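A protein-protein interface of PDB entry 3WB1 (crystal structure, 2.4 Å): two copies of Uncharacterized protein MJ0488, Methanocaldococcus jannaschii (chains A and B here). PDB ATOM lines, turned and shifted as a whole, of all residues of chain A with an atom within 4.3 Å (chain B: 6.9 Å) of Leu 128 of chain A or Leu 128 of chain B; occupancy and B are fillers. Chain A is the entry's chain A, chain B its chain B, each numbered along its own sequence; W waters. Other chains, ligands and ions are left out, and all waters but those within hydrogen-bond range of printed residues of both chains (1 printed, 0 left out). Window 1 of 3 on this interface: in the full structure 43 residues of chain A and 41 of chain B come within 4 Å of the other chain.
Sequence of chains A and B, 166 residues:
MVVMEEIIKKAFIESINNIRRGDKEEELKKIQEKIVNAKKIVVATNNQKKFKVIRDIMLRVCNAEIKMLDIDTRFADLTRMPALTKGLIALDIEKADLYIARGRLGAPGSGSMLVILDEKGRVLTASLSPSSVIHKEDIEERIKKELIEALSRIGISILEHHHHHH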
ATOM      1  N   LEU A 105      25.634 -18.997 -17.301  1.00  0.00           N
ATOM      2  CA  LEU A 105      24.324 -18.687 -17.866  1.00  0.00           C
ATOM      3  C   LEU A 105      23.400 -19.881 -17.761  1.00  0.00           C
ATOM      4  O   LEU A 105      22.333 -19.819 -17.137  1.00  0.00           O
ATOM      5  CB  LEU A 105      24.474 -18.286 -19.343  1.00  0.00           C
ATOM      6  CG  LEU A 105      23.424 -17.517 -20.169  1.00  0.00           C
ATOM      7  CD1 LEU A 105      23.469 -17.937 -21.635  1.00  0.00           C
ATOM      8  CD2 LEU A 105      22.011 -17.629 -19.630  1.00  0.00           C
ATOM      9  N   SER A 112      29.013 -16.852 -19.281  1.00  0.00           N
ATOM     10  CA  SER A 112      28.641 -16.282 -17.986  1.00  0.00           C
ATOM     11  C   SER A 112      27.552 -15.212 -18.028  1.00  0.00           C
ATOM     12  O   SER A 112      27.384 -14.489 -19.013  1.00  0.00           O
ATOM     13  CB  SER A 112      29.867 -15.688 -17.298  1.00  0.00           C
ATOM     14  OG  SER A 112      30.794 -16.703 -16.975  1.00  0.00           O
ATOM     15  N   MET A 113      26.837 -15.112 -16.916  1.00  0.00           N
ATOM     16  CA  MET A 113      25.810 -14.101 -16.723  1.00  0.00           C
ATOM     17  C   MET A 113      26.088 -13.359 -15.432  1.00  0.00           C
ATOM     18  O   MET A 113      26.477 -13.971 -14.433  1.00  0.00           O
ATOM     19  CB  MET A 113      24.418 -14.745 -16.683  1.00  0.00           C
ATOM     20  CG  MET A 113      23.319 -13.844 -16.111  1.00  0.00           C
ATOM     21  SD  MET A 113      21.705 -14.650 -15.949  1.00  0.00           S
ATOM     22  CE  MET A 113      20.922 -14.174 -17.484  1.00  0.00           C
ATOM     23  N   ALA A 126      20.551  -7.519 -16.280  1.00  0.00           N
ATOM     24  CA  ALA A 126      21.567  -8.557 -16.345  1.00  0.00           C
ATOM     25  C   ALA A 126      22.511  -8.263 -17.492  1.00  0.00           C
ATOM     26  O   ALA A 126      22.223  -7.412 -18.334  1.00  0.00           O
ATOM     27  CB  ALA A 126      20.926  -9.937 -16.519  1.00  0.00           C
ATOM     28  N   SER A 127      23.633  -8.970 -17.532  1.00  0.00           N
ATOM     29  CA  SER A 127      24.531  -8.896 -18.682  1.00  0.00           C
ATOM     30  C   SER A 127      25.225 -10.234 -18.879  1.00  0.00           C
ATOM     31  O   SER A 127      25.333 -11.035 -17.946  1.00  0.00           O
ATOM     32  CB  SER A 127      25.564  -7.782 -18.514  1.00  0.00           C
ATOM     33  OG  SER A 127      26.362  -8.014 -17.371  1.00  0.00           O
ATOM     34  N   LEU A 128      25.681 -10.472 -20.102  1.00  0.00           N
ATOM     35  CA  LEU A 128      26.300 -11.735 -20.462  1.00  0.00           C
ATOM     36  C   LEU A 128      27.712 -11.520 -20.992  1.00  0.00           C
ATOM     37  O   LEU A 128      28.063 -10.434 -21.456  1.00  0.00           O
ATOM     38  CB  LEU A 128      25.454 -12.478 -21.498  1.00  0.00           C
ATOM     39  CG  LEU A 128      23.967 -12.619 -21.164  1.00  0.00           C
ATOM     40  CD1 LEU A 128      23.203 -13.280 -22.306  1.00  0.00           C
ATOM     41  CD2 LEU A 128      23.803 -13.393 -19.866  1.00  0.00           C
ATOM     42  N   SER A 129      28.514 -12.573 -20.932  1.00  0.00           N
ATOM     43  CA  SER A 129      29.846 -12.540 -21.497  1.00  0.00           C
ATOM     44  C   SER A 129      30.084 -13.807 -22.286  1.00  0.00           C
ATOM     45  O   SER A 129      29.546 -14.861 -21.955  1.00  0.00           O
ATOM     46  CB  SER A 129      30.892 -12.396 -20.399  1.00  0.00           C
ATOM     47  OG  SER A 129      30.794 -11.120 -19.804  1.00  0.00           O
ATOM     48  N   ARG A 153      22.269  -0.409 -19.312  1.00  0.00           N
ATOM     49  CA  ARG A 153      21.125  -0.842 -20.109  1.00  0.00           C
ATOM     50  C   ARG A 153      19.789  -0.483 -19.439  1.00  0.00           C
ATOM     51  O   ARG A 153      18.758  -0.473 -20.109  1.00  0.00           O
ATOM     52  CB  ARG A 153      21.200  -2.349 -20.410  1.00  0.00           C
ATOM     53  CG  ARG A 153      21.050  -3.276 -19.202  1.00  0.00           C
ATOM     54  CD  ARG A 153      21.253  -4.734 -19.613  1.00  0.00           C
ATOM     55  NE  ARG A 153      20.211  -5.202 -20.532  1.00  0.00           N
ATOM     56  CZ  ARG A 153      19.019  -5.651 -20.143  1.00  0.00           C
ATOM     57  NH1 ARG A 153      18.126  -6.058 -21.042  1.00  0.00           N
ATOM     58  NH2 ARG A 153      18.716  -5.699 -18.851  1.00  0.00           N
ATOM     59  N   LEU B 105      13.339  -9.680 -20.502  1.00  0.00           N
ATOM     60  CA  LEU B 105      14.351 -10.363 -19.688  1.00  0.00           C
ATOM     61  C   LEU B 105      13.746 -10.879 -18.391  1.00  0.00           C
ATOM     62  O   LEU B 105      13.744 -12.089 -18.104  1.00  0.00           O
ATOM     63  CB  LEU B 105      15.493  -9.401 -19.355  1.00  0.00           C
ATOM     64  CG  LEU B 105      16.924  -9.838 -19.031  1.00  0.00           C
ATOM     65  CD1 LEU B 105      17.549  -8.880 -18.022  1.00  0.00           C
ATOM     66  CD2 LEU B 105      17.037 -11.274 -18.552  1.00  0.00           C
ATOM     67  N   SER B 110      13.323  -4.230 -17.832  1.00  0.00           N
ATOM     68  CA  SER B 110      14.598  -4.943 -17.807  1.00  0.00           C
ATOM     69  C   SER B 110      15.157  -5.154 -19.217  1.00  0.00           C
ATOM     70  O   SER B 110      16.199  -5.795 -19.387  1.00  0.00           O
ATOM     71  CB  SER B 110      14.468  -6.302 -17.092  1.00  0.00           C
ATOM     72  OG  SER B 110      13.457  -7.125 -17.655  1.00  0.00           O
ATOM     73  N   GLY B 111      14.426  -4.684 -20.223  1.00  0.00           N
ATOM     74  CA  GLY B 111      14.855  -4.837 -21.602  1.00  0.00           C
ATOM     75  C   GLY B 111      14.500  -6.214 -22.127  1.00  0.00           C
ATOM     76  O   GLY B 111      13.652  -6.897 -21.555  1.00  0.00           O
ATOM     77  N   SER B 112      15.151  -6.635 -23.206  1.00  0.00           N
ATOM     78  CA  SER B 112      14.747  -7.861 -23.883  1.00  0.00           C
ATOM     79  C   SER B 112      15.812  -8.958 -23.829  1.00  0.00           C
ATOM     80  O   SER B 112      17.008  -8.678 -23.755  1.00  0.00           O
ATOM     81  CB  SER B 112      14.388  -7.554 -25.334  1.00  0.00           C
ATOM     82  OG  SER B 112      13.257  -6.700 -25.393  1.00  0.00           O
ATOM     83  N   MET B 113      15.373 -10.211 -23.888  1.00  0.00           N
ATOM     84  CA  MET B 113      16.299 -11.340 -23.962  1.00  0.00           C
ATOM     85  C   MET B 113      15.949 -12.227 -25.146  1.00  0.00           C
ATOM     86  O   MET B 113      14.773 -12.490 -25.406  1.00  0.00           O
ATOM     87  CB  MET B 113      16.284 -12.167 -22.668  1.00  0.00           C
ATOM     88  CG  MET B 113      16.930 -13.548 -22.825  1.00  0.00           C
ATOM     89  SD  MET B 113      16.862 -14.664 -21.399  1.00  0.00           S
ATOM     90  CE  MET B 113      18.446 -14.351 -20.625  1.00  0.00           C
ATOM     91  N   LEU B 114      16.970 -12.644 -25.891  1.00  0.00           N
ATOM     92  CA  LEU B 114      16.817 -13.699 -26.889  1.00  0.00           C
ATOM     93  C   LEU B 114      17.521 -14.944 -26.373  1.00  0.00           C
ATOM     94  O   LEU B 114      18.676 -14.858 -25.961  1.00  0.00           O
ATOM     95  CB  LEU B 114      17.393 -13.272 -28.245  1.00  0.00           C
ATOM     96  CG  LEU B 114      17.253 -14.264 -29.406  1.00  0.00           C
ATOM     97  CD1 LEU B 114      17.035 -13.533 -30.722  1.00  0.00           C
ATOM     98  CD2 LEU B 114      18.472 -15.164 -29.501  1.00  0.00           C
ATOM     99  N   THR B 125      22.568 -20.662 -25.167  1.00  0.00           N
ATOM    100  CA  THR B 125      23.137 -19.327 -25.307  1.00  0.00           C
ATOM    101  C   THR B 125      22.017 -18.303 -25.312  1.00  0.00           C
ATOM    102  O   THR B 125      20.851 -18.663 -25.451  1.00  0.00           O
ATOM    103  CB  THR B 125      23.984 -19.178 -26.593  1.00  0.00           C
ATOM    104  OG1 THR B 125      24.631 -17.901 -26.588  1.00  0.00           O
ATOM    105  CG2 THR B 125      23.114 -19.307 -27.845  1.00  0.00           C
ATOM    106  N   ALA B 126      22.374 -17.033 -25.154  1.00  0.00           N
ATOM    107  CA  ALA B 126      21.395 -15.953 -25.117  1.00  0.00           C
ATOM    108  C   ALA B 126      22.059 -14.621 -25.419  1.00  0.00           C
ATOM    109  O   ALA B 126      23.282 -14.521 -25.430  1.00  0.00           O
ATOM    110  CB  ALA B 126      20.695 -15.901 -23.756  1.00  0.00           C
ATOM    111  N   SER B 127      21.242 -13.596 -25.636  1.00  0.00           N
ATOM    112  CA  SER B 127      21.739 -12.238 -25.801  1.00  0.00           C
ATOM    113  C   SER B 127      20.746 -11.243 -25.209  1.00  0.00           C
ATOM    114  O   SER B 127      19.565 -11.566 -25.040  1.00  0.00           O
ATOM    115  CB  SER B 127      21.982 -11.944 -27.278  1.00  0.00           C
ATOM    116  OG  SER B 127      20.777 -12.092 -28.008  1.00  0.00           O
ATOM    117  N   LEU B 128      21.231 -10.056 -24.847  1.00  0.00           N
ATOM    118  CA  LEU B 128      20.376  -9.052 -24.219  1.00  0.00           C
ATOM    119  C   LEU B 128      20.398  -7.732 -24.987  1.00  0.00           C
ATOM    120  O   LEU B 128      21.376  -7.413 -25.663  1.00  0.00           O
ATOM    121  CB  LEU B 128      20.800  -8.834 -22.757  1.00  0.00           C
ATOM    122  CG  LEU B 128      20.949 -10.101 -21.891  1.00  0.00           C
ATOM    123  CD1 LEU B 128      21.508  -9.786 -20.512  1.00  0.00           C
ATOM    124  CD2 LEU B 128      19.610 -10.789 -21.744  1.00  0.00           C
ATOM    125  N   SER B 129      19.327  -6.954 -24.869  1.00  0.00           N
ATOM    126  CA  SER B 129      19.301  -5.613 -25.444  1.00  0.00           C
ATOM    127  C   SER B 129      18.635  -4.642 -24.490  1.00  0.00           C
ATOM    128  O   SER B 129      17.741  -5.030 -23.733  1.00  0.00           O
ATOM    129  CB  SER B 129      18.573  -5.607 -26.788  1.00  0.00           C
ATOM    130  OG  SER B 129      19.313  -6.317 -27.763  1.00  0.00           O
ATOM    131  N   PRO B 130      19.057  -3.371 -24.528  1.00  0.00           N
ATOM    132  CA  PRO B 130      18.403  -2.366 -23.690  1.00  0.00           C
ATOM    133  C   PRO B 130      16.952  -2.146 -24.097  1.00  0.00           C
ATOM    134  O   PRO B 130      16.573  -2.446 -25.235  1.00  0.00           O
ATOM    135  CB  PRO B 130      19.233  -1.096 -23.941  1.00  0.00           C
ATOM    136  CG  PRO B 130      20.541  -1.589 -24.487  1.00  0.00           C
ATOM    137  CD  PRO B 130      20.207  -2.821 -25.264  1.00  0.00           C
ATOM    138  N   LYS B 145      20.970  -8.380 -34.499  1.00  0.00           N
ATOM    139  CA  LYS B 145      22.127  -8.177 -33.638  1.00  0.00           C
ATOM    140  C   LYS B 145      22.091  -9.129 -32.450  1.00  0.00           C
ATOM    141  O   LYS B 145      23.126  -9.638 -32.012  1.00  0.00           O
ATOM    142  CB  LYS B 145      22.175  -6.738 -33.124  1.00  0.00           C
ATOM    143  CG  LYS B 145      23.321  -6.490 -32.153  1.00  0.00           C
ATOM    144  CD  LYS B 145      22.980  -5.453 -31.079  1.00  0.00           C
ATOM    145  CE  LYS B 145      22.023  -6.029 -30.032  1.00  0.00           C
ATOM    146  NZ  LYS B 145      21.908  -5.173 -28.816  1.00  0.00           N
ATOM    147  N   GLU B 146      20.895  -9.352 -31.918  1.00  0.00           N
ATOM    148  CA  GLU B 146      20.731 -10.273 -30.802  1.00  0.00           C
ATOM    149  C   GLU B 146      21.135 -11.682 -31.193  1.00  0.00           C
ATOM    150  O   GLU B 146      21.923 -12.316 -30.492  1.00  0.00           O
ATOM    151  CB  GLU B 146      19.286 -10.258 -30.301  1.00  0.00           C
ATOM    152  CG  GLU B 146      18.933  -9.005 -29.517  1.00  0.00           C
ATOM    153  CD  GLU B 146      17.443  -8.831 -29.325  1.00  0.00           C
ATOM    154  OE1 GLU B 146      16.675  -9.758 -29.676  1.00  0.00           O
ATOM    155  OE2 GLU B 146      17.041  -7.757 -28.821  1.00  0.00           O
ATOM    156  N   GLU B 149      25.000 -12.081 -31.894  1.00  0.00           N
ATOM    157  CA  GLU B 149      25.797 -12.106 -30.665  1.00  0.00           C
ATOM    158  C   GLU B 149      25.612 -13.428 -29.924  1.00  0.00           C
ATOM    159  O   GLU B 149      26.576 -14.007 -29.417  1.00  0.00           O
ATOM    160  CB  GLU B 149      25.427 -10.947 -29.730  1.00  0.00           C
ATOM    161  CG  GLU B 149      26.345 -10.840 -28.504  1.00  0.00           C
ATOM    162  CD  GLU B 149      25.982  -9.689 -27.572  1.00  0.00           C
ATOM    163  OE1 GLU B 149      24.930  -9.044 -27.788  1.00  0.00           O
ATOM    164  OE2 GLU B 149      26.757  -9.427 -26.622  1.00  0.00           O
ATOM    165  N   ARG B 153      28.984 -15.487 -29.453  1.00  0.00           N
ATOM    166  CA  ARG B 153      29.556 -15.618 -28.118  1.00  0.00           C
ATOM    167  C   ARG B 153      29.867 -17.075 -27.767  1.00  0.00           C
ATOM    168  O   ARG B 153      30.641 -17.336 -26.841  1.00  0.00           O
ATOM    169  CB  ARG B 153      28.609 -15.019 -27.072  1.00  0.00           C
ATOM    170  CG  ARG B 153      27.292 -15.775 -26.943  1.00  0.00           C
ATOM    171  CD  ARG B 153      26.344 -15.079 -25.976  1.00  0.00           C
ATOM    172  NE  ARG B 153      26.872 -15.119 -24.615  1.00  0.00           N
ATOM    173  CZ  ARG B 153      26.731 -16.155 -23.793  1.00  0.00           C
ATOM    174  NH1 ARG B 153      26.066 -17.238 -24.189  1.00  0.00           N
ATOM    175  NH2 ARG B 153      27.251 -16.110 -22.573  1.00  0.00           N
HETATM  176  O   HOH W   1      21.570  -5.144 -22.982  1.00  0.00           O
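O of Ser 129 of chain A sits at hydrogen-bond distance from NH2 of Arg 153 of chain B (2.7 Å). The guanidinium group of Arg 153 of chain A sits at hydrogen-bond distance from the backbone carbonyl oxygen of Ser 110 of chain B, 2.6 Å away. O of Ser 129 of chain B lies within hydrogen-bond range of NH1 of Arg 153 of chain A.
The backbone NH (N) of Ser 127 of chain B sits at hydrogen-bond distance from the backbone carbonyl oxygen (O) of Leu 114 of chain B (2.9 Å). N of Ser 112 of chain B lies within hydrogen-bond range of O of Ser 129 of chain B. The side-chain hydroxyl (OG) of Ser 129 of chain B is in hydrogen-bond range of the side-chain carboxylate (OE2) of Glu 146 of chain B (2.9 Å). The backbone carbonyl oxygen (O) of Ser 112 of chain A lies within hydrogen-bond range of the backbone NH (N) of Ser 129 of chain A (2.9 Å). The backbone carbonyl oxygen of Gly 111 of chain B sits at hydrogen-bond distance from the backbone NH of Leu 105 of chain B (3.0 Å). OG of Ser 129 of chain B sits at hydrogen-bond distance from NZ of Lys 145 of chain B, 3.0 Å away.
Leu 105 of chain A touches Thr 125 of chain B. CD1 of Leu 105 of chain A touches N of Ala 126 of chain B, at 3.8 Å. Leu 105 of chain A touches Arg 153 of chain B. N of Ser 112 of chain A touches NH2 of Arg 153 of chain B, at 3.8 Å. Leu 128 of chain B touches Ala 126 of chain A (CD1 to O, 3.3 Å). Leu 128 of chain B touches Ser 127 of chain A (CD1 to CA, 3.6 Å). Leu 128 of chain A touches Leu 128 of chain B. Gly 111 of chain B touches Arg 153 of chain A. Arg 153 of chain A touches Ser 112 of chain B. Arg 153 of chain A touches Pro 130 of chain B.
Printed residues of chain B within 4 Å of Leu 128 of chain A: Ala 126 (3.4 Å), Ser 127 (3.9 Å) and Leu 128 (3.8 Å). Leu 128 of chain B touches just these residues of chain A: Ala 126 (3.3 Å), Ser 127 (3.6 Å) and Leu 128 (3.8 Å). Of the printed residues of chain A, Ala 126 of chain B touches Leu 105 and Leu 128. Of the printed residues of chain B, Leu 105 of chain A touches Thr 125, Ala 126 and Arg 153. Leu 114 of chain B touches none of the printed residues of chain A. The nearest residue of chain B that does not touch Leu 128 of chain A is Arg 153 of chain B (4.2 Å). The nearest printed residue of chain A that does not touch Gly 111 of chain B is Ala 126 of chain A (7.8 Å).
Printed residues of chain B that touch a printed residue of chain A: Leu 105, Ser 110, Gly 111, Ser 112, Thr 125, Ala 126, Ser 127, Leu 128, Ser 129, Pro 130 and Arg 153. Along chain B the printed residues that touch a printed residue of chain A span positions 105 to 153. Of the 8 printed residues of chain A, 7 touch a printed residue of chain B. Hydrophobic or aromatic side chains of chain A within 4 Å of the printed part of chain B: Leu 105, Ala 126 and Leu 128. Among the printed residues, 17 pairs touch across the chains.
Leu 105 of chain A touches Ala 126 of chain B, and with the chains exchanged Ala 126 of chain A touches Leu 105 of chain B. Ser 112 of chain A touches Arg 153 of chain B, and with the chains exchanged Arg 153 of chain A touches Ser 112 of chain B. Ala 126 of chain A touches Leu 128 of chain B, and with the chains exchanged Leu 128 of chain A touches Ala 126 of chain B. Leu 128 of chain A touches its own counterpart, Leu 128 of chain B. Positions printed for both chains: 105, 112, 113, 126, 127, 128, 129 and 153. Of the 17 pairs that touch across the chains among the printed residues, 13 have their exchanged pair printed and touching as well.
Water W1 lies within hydrogen-bond range of NE of Arg 153 of chain A (2.8 Å) and N of Ser 129 of chain B (3.4 Å).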
